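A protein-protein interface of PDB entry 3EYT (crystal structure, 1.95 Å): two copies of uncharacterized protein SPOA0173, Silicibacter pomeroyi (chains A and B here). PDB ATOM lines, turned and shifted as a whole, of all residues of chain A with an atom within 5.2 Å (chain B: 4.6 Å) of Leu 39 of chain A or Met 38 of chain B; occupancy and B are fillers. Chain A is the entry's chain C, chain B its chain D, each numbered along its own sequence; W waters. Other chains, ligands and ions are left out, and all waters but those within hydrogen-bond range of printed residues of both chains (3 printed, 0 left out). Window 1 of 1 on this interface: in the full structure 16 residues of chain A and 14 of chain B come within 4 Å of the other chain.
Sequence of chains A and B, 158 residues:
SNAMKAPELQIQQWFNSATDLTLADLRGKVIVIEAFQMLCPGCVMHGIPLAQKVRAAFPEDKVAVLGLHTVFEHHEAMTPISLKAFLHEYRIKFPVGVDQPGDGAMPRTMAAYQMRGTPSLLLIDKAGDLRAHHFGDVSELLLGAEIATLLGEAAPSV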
ATOM      1  N   GLN A  37      -5.562  15.935  -3.354  1.00  0.00           N
ATOM      2  CA  GLN A  37      -5.561  16.551  -2.028  1.00  0.00           C
ATOM      3  C   GLN A  37      -4.581  15.737  -1.227  1.00  0.00           C
ATOM      4  O   GLN A  37      -4.601  14.489  -1.283  1.00  0.00           O
ATOM      5  CB  GLN A  37      -6.925  16.415  -1.328  1.00  0.00           C
ATOM      6  CG  GLN A  37      -8.071  17.227  -1.976  1.00  0.00           C
ATOM      7  CD  GLN A  37      -9.354  17.177  -1.146  1.00  0.00           C
ATOM      8  OE1 GLN A  37      -9.750  18.177  -0.578  1.00  0.00           O
ATOM      9  NE2 GLN A  37      -9.948  15.999  -1.018  1.00  0.00           N
ATOM     10  N   MET A  38      -3.767  16.425  -0.442  1.00  0.00           N
ATOM     11  CA  MET A  38      -2.695  15.769   0.301  1.00  0.00           C
ATOM     12  C   MET A  38      -3.216  14.783   1.350  1.00  0.00           C
ATOM     13  O   MET A  38      -2.548  13.812   1.645  1.00  0.00           O
ATOM     14  CB  MET A  38      -1.769  16.813   0.927  1.00  0.00           C
ATOM     15  CG  MET A  38      -2.482  17.700   1.947  1.00  0.00           C
ATOM     16  SD  MET A  38      -1.227  18.996   2.705  1.00  0.00           S
ATOM     17  CE  MET A  38      -0.431  17.831   4.097  1.00  0.00           C
ATOM     18  N   LEU A  39      -4.407  15.014   1.901  1.00  0.00           N
ATOM     19  CA  LEU A  39      -4.966  14.091   2.896  1.00  0.00           C
ATOM     20  C   LEU A  39      -5.955  13.041   2.331  1.00  0.00           C
ATOM     21  O   LEU A  39      -6.634  12.328   3.076  1.00  0.00           O
ATOM     22  CB  LEU A  39      -5.610  14.889   4.057  1.00  0.00           C
ATOM     23  CG  LEU A  39      -4.732  15.911   4.793  1.00  0.00           C
ATOM     24  CD1 LEU A  39      -5.532  16.497   5.957  1.00  0.00           C
ATOM     25  CD2 LEU A  39      -3.423  15.256   5.319  1.00  0.00           C
ATOM     26  N   CYS A  40      -6.017  12.920   1.017  1.00  0.00           N
ATOM     27  CA  CYS A  40      -6.921  11.964   0.408  1.00  0.00           C
ATOM     28  C   CYS A  40      -6.186  10.638   0.217  1.00  0.00           C
ATOM     29  O   CYS A  40      -5.171  10.587  -0.467  1.00  0.00           O
ATOM     30  CB  CYS A  40      -7.436  12.554  -0.896  1.00  0.00           C
ATOM     31  SG  CYS A  40      -8.034  11.387  -2.126  1.00  0.00           S
ATOM     32  N   PRO A  41      -6.673   9.564   0.862  1.00  0.00           N
ATOM     33  CA  PRO A  41      -5.878   8.325   0.860  1.00  0.00           C
ATOM     34  C   PRO A  41      -5.610   7.786  -0.545  1.00  0.00           C
ATOM     35  O   PRO A  41      -4.508   7.292  -0.800  1.00  0.00           O
ATOM     36  CB  PRO A  41      -6.708   7.342   1.711  1.00  0.00           C
ATOM     37  CG  PRO A  41      -7.548   8.229   2.582  1.00  0.00           C
ATOM     38  CD  PRO A  41      -7.835   9.483   1.762  1.00  0.00           C
ATOM     39  N   ALA A  77      -6.753  22.237   7.074  1.00  0.00           N
ATOM     40  CA  ALA A  77      -5.851  21.128   7.348  1.00  0.00           C
ATOM     41  C   ALA A  77      -4.802  20.959   6.258  1.00  0.00           C
ATOM     42  O   ALA A  77      -3.811  20.243   6.482  1.00  0.00           O
ATOM     43  CB  ALA A  77      -6.628  19.865   7.442  1.00  0.00           C
ATOM     44  N   MET A  78      -5.046  21.579   5.090  1.00  0.00           N
ATOM     45  CA  MET A  78      -4.296  21.318   3.862  1.00  0.00           C
ATOM     46  C   MET A  78      -3.787  22.626   3.248  1.00  0.00           C
ATOM     47  O   MET A  78      -3.796  22.774   2.024  1.00  0.00           O
ATOM     48  CB  MET A  78      -5.171  20.597   2.845  1.00  0.00           C
ATOM     49  CG  MET A  78      -5.753  19.258   3.369  1.00  0.00           C
ATOM     50  SD  MET A  78      -6.309  18.158   1.913  1.00  0.00           S
ATOM     51  CE  MET A  78      -8.078  17.674   2.586  1.00  0.00           C
ATOM     52  N   TYR A  90       7.322  13.134   0.918  1.00  0.00           N
ATOM     53  CA  TYR A  90       7.027  12.182  -0.126  1.00  0.00           C
ATOM     54  C   TYR A  90       7.920  12.365  -1.350  1.00  0.00           C
ATOM     55  O   TYR A  90       7.663  11.759  -2.403  1.00  0.00           O
ATOM     56  CB  TYR A  90       5.560  12.300  -0.517  1.00  0.00           C
ATOM     57  CG  TYR A  90       4.671  11.625   0.495  1.00  0.00           C
ATOM     58  CD1 TYR A  90       4.238  12.304   1.647  1.00  0.00           C
ATOM     59  CD2 TYR A  90       4.284  10.299   0.316  1.00  0.00           C
ATOM     60  CE1 TYR A  90       3.453  11.660   2.585  1.00  0.00           C
ATOM     61  CE2 TYR A  90       3.504   9.645   1.264  1.00  0.00           C
ATOM     62  CZ  TYR A  90       3.072  10.340   2.365  1.00  0.00           C
ATOM     63  OH  TYR A  90       2.275   9.696   3.279  1.00  0.00           O
ATOM     64  N   PHE B  36       3.395   7.891  15.680  1.00  0.00           N
ATOM     65  CA  PHE B  36       3.409   8.164  14.249  1.00  0.00           C
ATOM     66  C   PHE B  36       3.402   9.676  13.997  1.00  0.00           C
ATOM     67  O   PHE B  36       3.113  10.461  14.923  1.00  0.00           O
ATOM     68  CB  PHE B  36       2.202   7.498  13.571  1.00  0.00           C
ATOM     69  CG  PHE B  36       0.907   8.236  13.778  1.00  0.00           C
ATOM     70  CD1 PHE B  36       0.428   9.117  12.812  1.00  0.00           C
ATOM     71  CD2 PHE B  36       0.177   8.063  14.964  1.00  0.00           C
ATOM     72  CE1 PHE B  36      -0.786   9.796  13.014  1.00  0.00           C
ATOM     73  CE2 PHE B  36      -1.016   8.741  15.186  1.00  0.00           C
ATOM     74  CZ  PHE B  36      -1.498   9.603  14.234  1.00  0.00           C
ATOM     75  N   GLN B  37       3.762  10.065  12.770  1.00  0.00           N
ATOM     76  CA  GLN B  37       3.571  11.440  12.287  1.00  0.00           C
ATOM     77  C   GLN B  37       2.712  11.314  11.046  1.00  0.00           C
ATOM     78  O   GLN B  37       2.948  10.416  10.226  1.00  0.00           O
ATOM     79  CB  GLN B  37       4.874  12.093  11.878  1.00  0.00           C
ATOM     80  CG  GLN B  37       5.711  12.516  13.058  1.00  0.00           C
ATOM     81  CD  GLN B  37       7.002  13.166  12.606  1.00  0.00           C
ATOM     82  OE1 GLN B  37       7.332  14.286  13.042  1.00  0.00           O
ATOM     83  NE2 GLN B  37       7.732  12.486  11.696  1.00  0.00           N
ATOM     84  N   MET B  38       1.709  12.175  10.921  1.00  0.00           N
ATOM     85  CA  MET B  38       0.700  12.024   9.827  1.00  0.00           C
ATOM     86  C   MET B  38       1.273  12.227   8.421  1.00  0.00           C
ATOM     87  O   MET B  38       0.652  11.799   7.401  1.00  0.00           O
ATOM     88  CB  MET B  38      -0.465  12.977  10.059  1.00  0.00           C
ATOM     89  CG  MET B  38      -0.004  14.420  10.143  1.00  0.00           C
ATOM     90  SD  MET B  38      -1.533  15.649  10.344  1.00  0.00           S
ATOM     91  CE  MET B  38      -2.096  15.743   8.444  1.00  0.00           C
ATOM     92  N   LEU B  39       2.439  12.876   8.343  1.00  0.00           N
ATOM     93  CA  LEU B  39       3.061  13.132   7.046  1.00  0.00           C
ATOM     94  C   LEU B  39       4.240  12.227   6.788  1.00  0.00           C
ATOM     95  O   LEU B  39       4.983  12.426   5.816  1.00  0.00           O
ATOM     96  CB  LEU B  39       3.485  14.617   6.900  1.00  0.00           C
ATOM     97  CG  LEU B  39       2.350  15.630   6.911  1.00  0.00           C
ATOM     98  CD1 LEU B  39       2.929  17.000   6.574  1.00  0.00           C
ATOM     99  CD2 LEU B  39       1.216  15.227   5.933  1.00  0.00           C
ATOM    100  N   CYS B  40       4.424  11.245   7.655  1.00  0.00           N
ATOM    101  CA  CYS B  40       5.499  10.280   7.507  1.00  0.00           C
ATOM    102  C   CYS B  40       5.029   9.100   6.616  1.00  0.00           C
ATOM    103  O   CYS B  40       4.102   8.382   6.973  1.00  0.00           O
ATOM    104  CB  CYS B  40       5.939   9.850   8.920  1.00  0.00           C
ATOM    105  SG  CYS B  40       7.027   8.382   8.981  1.00  0.00           S
ATOM    106  N   VAL B  44       1.977   6.134   7.348  1.00  0.00           N
ATOM    107  CA  VAL B  44       0.735   6.037   6.596  1.00  0.00           C
ATOM    108  C   VAL B  44       0.620   4.673   5.894  1.00  0.00           C
ATOM    109  O   VAL B  44      -0.427   4.036   5.949  1.00  0.00           O
ATOM    110  CB  VAL B  44       0.593   7.233   5.621  1.00  0.00           C
ATOM    111  CG1 VAL B  44      -0.577   7.046   4.684  1.00  0.00           C
ATOM    112  CG2 VAL B  44       0.459   8.530   6.435  1.00  0.00           C
ATOM    113  N   HIS B  69       0.484  10.908  18.310  1.00  0.00           N
ATOM    114  CA  HIS B  69       1.029  11.742  17.250  1.00  0.00           C
ATOM    115  C   HIS B  69       2.237  12.501  17.787  1.00  0.00           C
ATOM    116  O   HIS B  69       2.085  13.471  18.518  1.00  0.00           O
ATOM    117  CB  HIS B  69      -0.035  12.695  16.711  1.00  0.00           C
ATOM    118  CG  HIS B  69       0.282  13.257  15.356  1.00  0.00           C
ATOM    119  ND1 HIS B  69       0.068  14.581  15.041  1.00  0.00           N
ATOM    120  CD2 HIS B  69       0.739  12.667  14.222  1.00  0.00           C
ATOM    121  CE1 HIS B  69       0.405  14.790  13.779  1.00  0.00           C
ATOM    122  NE2 HIS B  69       0.823  13.647  13.260  1.00  0.00           N
ATOM    123  N   MET B  78       1.856  19.967  10.828  1.00  0.00           N
ATOM    124  CA  MET B  78       1.098  18.808  11.301  1.00  0.00           C
ATOM    125  C   MET B  78       0.403  19.075  12.608  1.00  0.00           C
ATOM    126  O   MET B  78       0.408  18.220  13.491  1.00  0.00           O
ATOM    127  CB  MET B  78       1.999  17.563  11.448  1.00  0.00           C
ATOM    128  CG  MET B  78       2.809  17.161  10.244  1.00  0.00           C
ATOM    129  SD  MET B  78       3.765  15.491  10.736  1.00  0.00           S
ATOM    130  CE  MET B  78       5.554  15.948  10.190  1.00  0.00           C
ATOM    131  N   SER B  82      -4.614  19.866  11.423  1.00  0.00           N
ATOM    132  CA  SER B  82      -4.417  18.946  10.273  1.00  0.00           C
ATOM    133  C   SER B  82      -4.685  17.485  10.703  1.00  0.00           C
ATOM    134  O   SER B  82      -5.249  16.684   9.949  1.00  0.00           O
ATOM    135  CB  SER B  82      -3.033  19.101   9.640  1.00  0.00           C
ATOM    136  OG  SER B  82      -2.800  20.412   9.093  1.00  0.00           O
ATOM    137  N   LEU B  83      -4.312  17.147  11.932  1.00  0.00           N
ATOM    138  CA  LEU B  83      -4.552  15.789  12.432  1.00  0.00           C
ATOM    139  C   LEU B  83      -6.048  15.478  12.486  1.00  0.00           C
ATOM    140  O   LEU B  83      -6.450  14.386  12.109  1.00  0.00           O
ATOM    141  CB  LEU B  83      -3.929  15.582  13.820  1.00  0.00           C
ATOM    142  CG  LEU B  83      -3.991  14.160  14.389  1.00  0.00           C
ATOM    143  CD1 LEU B  83      -3.190  13.137  13.549  1.00  0.00           C
ATOM    144  CD2 LEU B  83      -3.584  14.105  15.906  1.00  0.00           C
ATOM    145  N   ALA B  85      -8.418  16.388  10.570  1.00  0.00           N
ATOM    146  CA  ALA B  85      -8.888  16.077   9.207  1.00  0.00           C
ATOM    147  C   ALA B  85      -8.308  14.737   8.738  1.00  0.00           C
ATOM    148  O   ALA B  85      -9.004  13.911   8.132  1.00  0.00           O
ATOM    149  CB  ALA B  85      -8.481  17.191   8.262  1.00  0.00           C
ATOM    150  N   PHE B  86      -7.026  14.524   9.012  1.00  0.00           N
ATOM    151  CA  PHE B  86      -6.346  13.255   8.661  1.00  0.00           C
ATOM    152  C   PHE B  86      -7.047  12.017   9.251  1.00  0.00           C
ATOM    153  O   PHE B  86      -7.254  11.016   8.566  1.00  0.00           O
ATOM    154  CB  PHE B  86      -4.890  13.307   9.170  1.00  0.00           C
ATOM    155  CG  PHE B  86      -4.130  12.017   9.035  1.00  0.00           C
ATOM    156  CD1 PHE B  86      -3.459  11.719   7.863  1.00  0.00           C
ATOM    157  CD2 PHE B  86      -4.021  11.141  10.114  1.00  0.00           C
ATOM    158  CE1 PHE B  86      -2.704  10.552   7.745  1.00  0.00           C
ATOM    159  CE2 PHE B  86      -3.286   9.960  10.006  1.00  0.00           C
ATOM    160  CZ  PHE B  86      -2.628   9.670   8.812  1.00  0.00           C
ATOM    161  N   GLU B  89     -10.318  11.572   7.289  1.00  0.00           N
ATOM    162  CA  GLU B  89     -10.067  11.058   5.914  1.00  0.00           C
ATOM    163  C   GLU B  89      -9.642   9.587   5.944  1.00  0.00           C
ATOM    164  O   GLU B  89     -10.127   8.788   5.142  1.00  0.00           O
ATOM    165  CB  GLU B  89      -8.985  11.880   5.189  1.00  0.00           C
ATOM    166  CG  GLU B  89      -9.383  13.323   4.845  1.00  0.00           C
ATOM    167  CD  GLU B  89     -10.101  13.472   3.502  1.00  0.00           C
ATOM    168  OE1 GLU B  89     -10.559  12.445   2.919  1.00  0.00           O
ATOM    169  OE2 GLU B  89     -10.188  14.638   3.013  1.00  0.00           O
ATOM    170  N   TYR B  90      -8.734   9.232   6.850  1.00  0.00           N
ATOM    171  CA  TYR B  90      -8.267   7.859   6.908  1.00  0.00           C
ATOM    172  C   TYR B  90      -9.162   6.958   7.771  1.00  0.00           C
ATOM    173  O   TYR B  90      -8.850   5.787   7.939  1.00  0.00           O
ATOM    174  CB  TYR B  90      -6.791   7.776   7.377  1.00  0.00           C
ATOM    175  CG  TYR B  90      -5.816   8.147   6.287  1.00  0.00           C
ATOM    176  CD1 TYR B  90      -5.575   9.492   5.977  1.00  0.00           C
ATOM    177  CD2 TYR B  90      -5.176   7.163   5.531  1.00  0.00           C
ATOM    178  CE1 TYR B  90      -4.696   9.854   4.952  1.00  0.00           C
ATOM    179  CE2 TYR B  90      -4.275   7.512   4.492  1.00  0.00           C
ATOM    180  CZ  TYR B  90      -4.048   8.859   4.221  1.00  0.00           C
ATOM    181  OH  TYR B  90      -3.163   9.244   3.238  1.00  0.00           O
HETATM  182  O   HOH W   1      -2.847   6.814   1.696  1.00  0.00           O
HETATM  183  O   HOH W   2      -2.106  11.653   3.828  1.00  0.00           O
HETATM  184  O   HOH W   3       0.622  11.585   4.718  1.00  0.00           O
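OG of Ser 82 of chain B lies within hydrogen-bond range of O of Ala 77 of chain A.
The backbone NH of Leu 39 of chain A sits at hydrogen-bond distance from the side-chain sulfur of Met 78 of chain A, 3.7 Å away. NE2 of His 69 of chain B lies within hydrogen-bond range of N of Met 38 of chain B (2.9 Å). The backbone NH of Leu 83 of chain B is in hydrogen-bond range of the side-chain sulfur of Met 38 of chain B. The side-chain sulfur (SD) of Met 78 of chain B is in hydrogen-bond range of the backbone NH (N) of Leu 39 of chain B, at 3.8 Å.
Among the printed residues, pairs that only touch across the chains: Leu 39 of chain A with Glu 89 of chain B (3.2 Å), Ala 77 of chain A with Ala 85 of chain B (3.4 Å), Leu 39 of chain A with Met 38 of chain B (3.4 Å), Met 38 of chain A with Leu 39 of chain B (3.6 Å), Tyr 90 of chain A with Leu 39 of chain B (3.7 Å), Leu 39 of chain A with Tyr 90 of chain B (3.7 Å), Pro 41 of chain A with Glu 89 of chain B (3.7 Å), Pro 41 of chain A with Tyr 90 of chain B (3.7 Å), Met 78 of chain A with Glu 89 of chain B (3.7 Å), Tyr 90 of chain A with Val 44 of chain B (3.8 Å), Leu 39 of chain A with Ala 85 of chain B (3.8 Å) and Leu 39 of chain A with Phe 86 of chain B (3.9 Å).
Printed residues of chain B within 4 Å of Met 38 of chain A: Leu 39 (3.6 Å). Printed residues of chain B within 4 Å of Leu 39 of chain A: Met 38, Ala 85, Phe 86, Glu 89 and Tyr 90. Met 38 of chain B touches just one residue of chain A: Leu 39 (3.4 Å). Printed residues of chain A within 4 Å of Val 44 of chain B: Tyr 90. Met 78 of chain B touches none of the printed residues of chain A. Of the printed residues of chain A, Glu 89 of chain B touches Leu 39 (3.2 Å), Pro 41 (3.7 Å) and Met 78 (3.7 Å).
Of the 14 printed residues of chain B, 8 touch a printed residue of chain A. Printed residues of chain B that touch a printed residue of chain A: Met 38, Leu 39, Val 44, Ser 82, Ala 85, Phe 86, Glu 89 and Tyr 90. Hydrophobic or aromatic side chains of chain B that line the printed part of chain A: Met 38, Leu 39, Val 44, Ala 85 and Tyr 90. Of the 8 printed residues of chain A, 6 touch a printed residue of chain B. Hydrophobic or aromatic side chains of chain A within 4 Å of the printed part of chain B: Met 38, Leu 39, Pro 41, Ala 77, Met 78 and Tyr 90. Along chain A the printed residues that touch a printed residue of chain B span positions 38 to 90.
Met 38 of chain A touches Leu 39 of chain B, and with the chains exchanged Leu 39 of chain A touches Met 38 of chain B. Leu 39 of chain A touches Tyr 90 of chain B, and with the chains exchanged Tyr 90 of chain A touches Leu 39 of chain B. Positions printed for both chains: 37, 38, 39, 40, 78 and 90. Of the 13 pairs that touch across the chains among the printed residues, 4 have their exchanged pair printed and touching as well.
Water W3 lies within hydrogen-bond range of the backbone carbonyl oxygen (O) of Met 38 of chain B and the side-chain hydroxyl (OH) of Tyr 90 of chain A. Water W2 lies within hydrogen-bond range of the side-chain hydroxyl (OH) of Tyr 90 of chain B and the backbone carbonyl oxygen (O) of Met 38 of chain A. Water W1 bridges OH of Tyr 90 of chain B (2.9 Å) and O of Pro 41 of chain A (3.0 Å).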
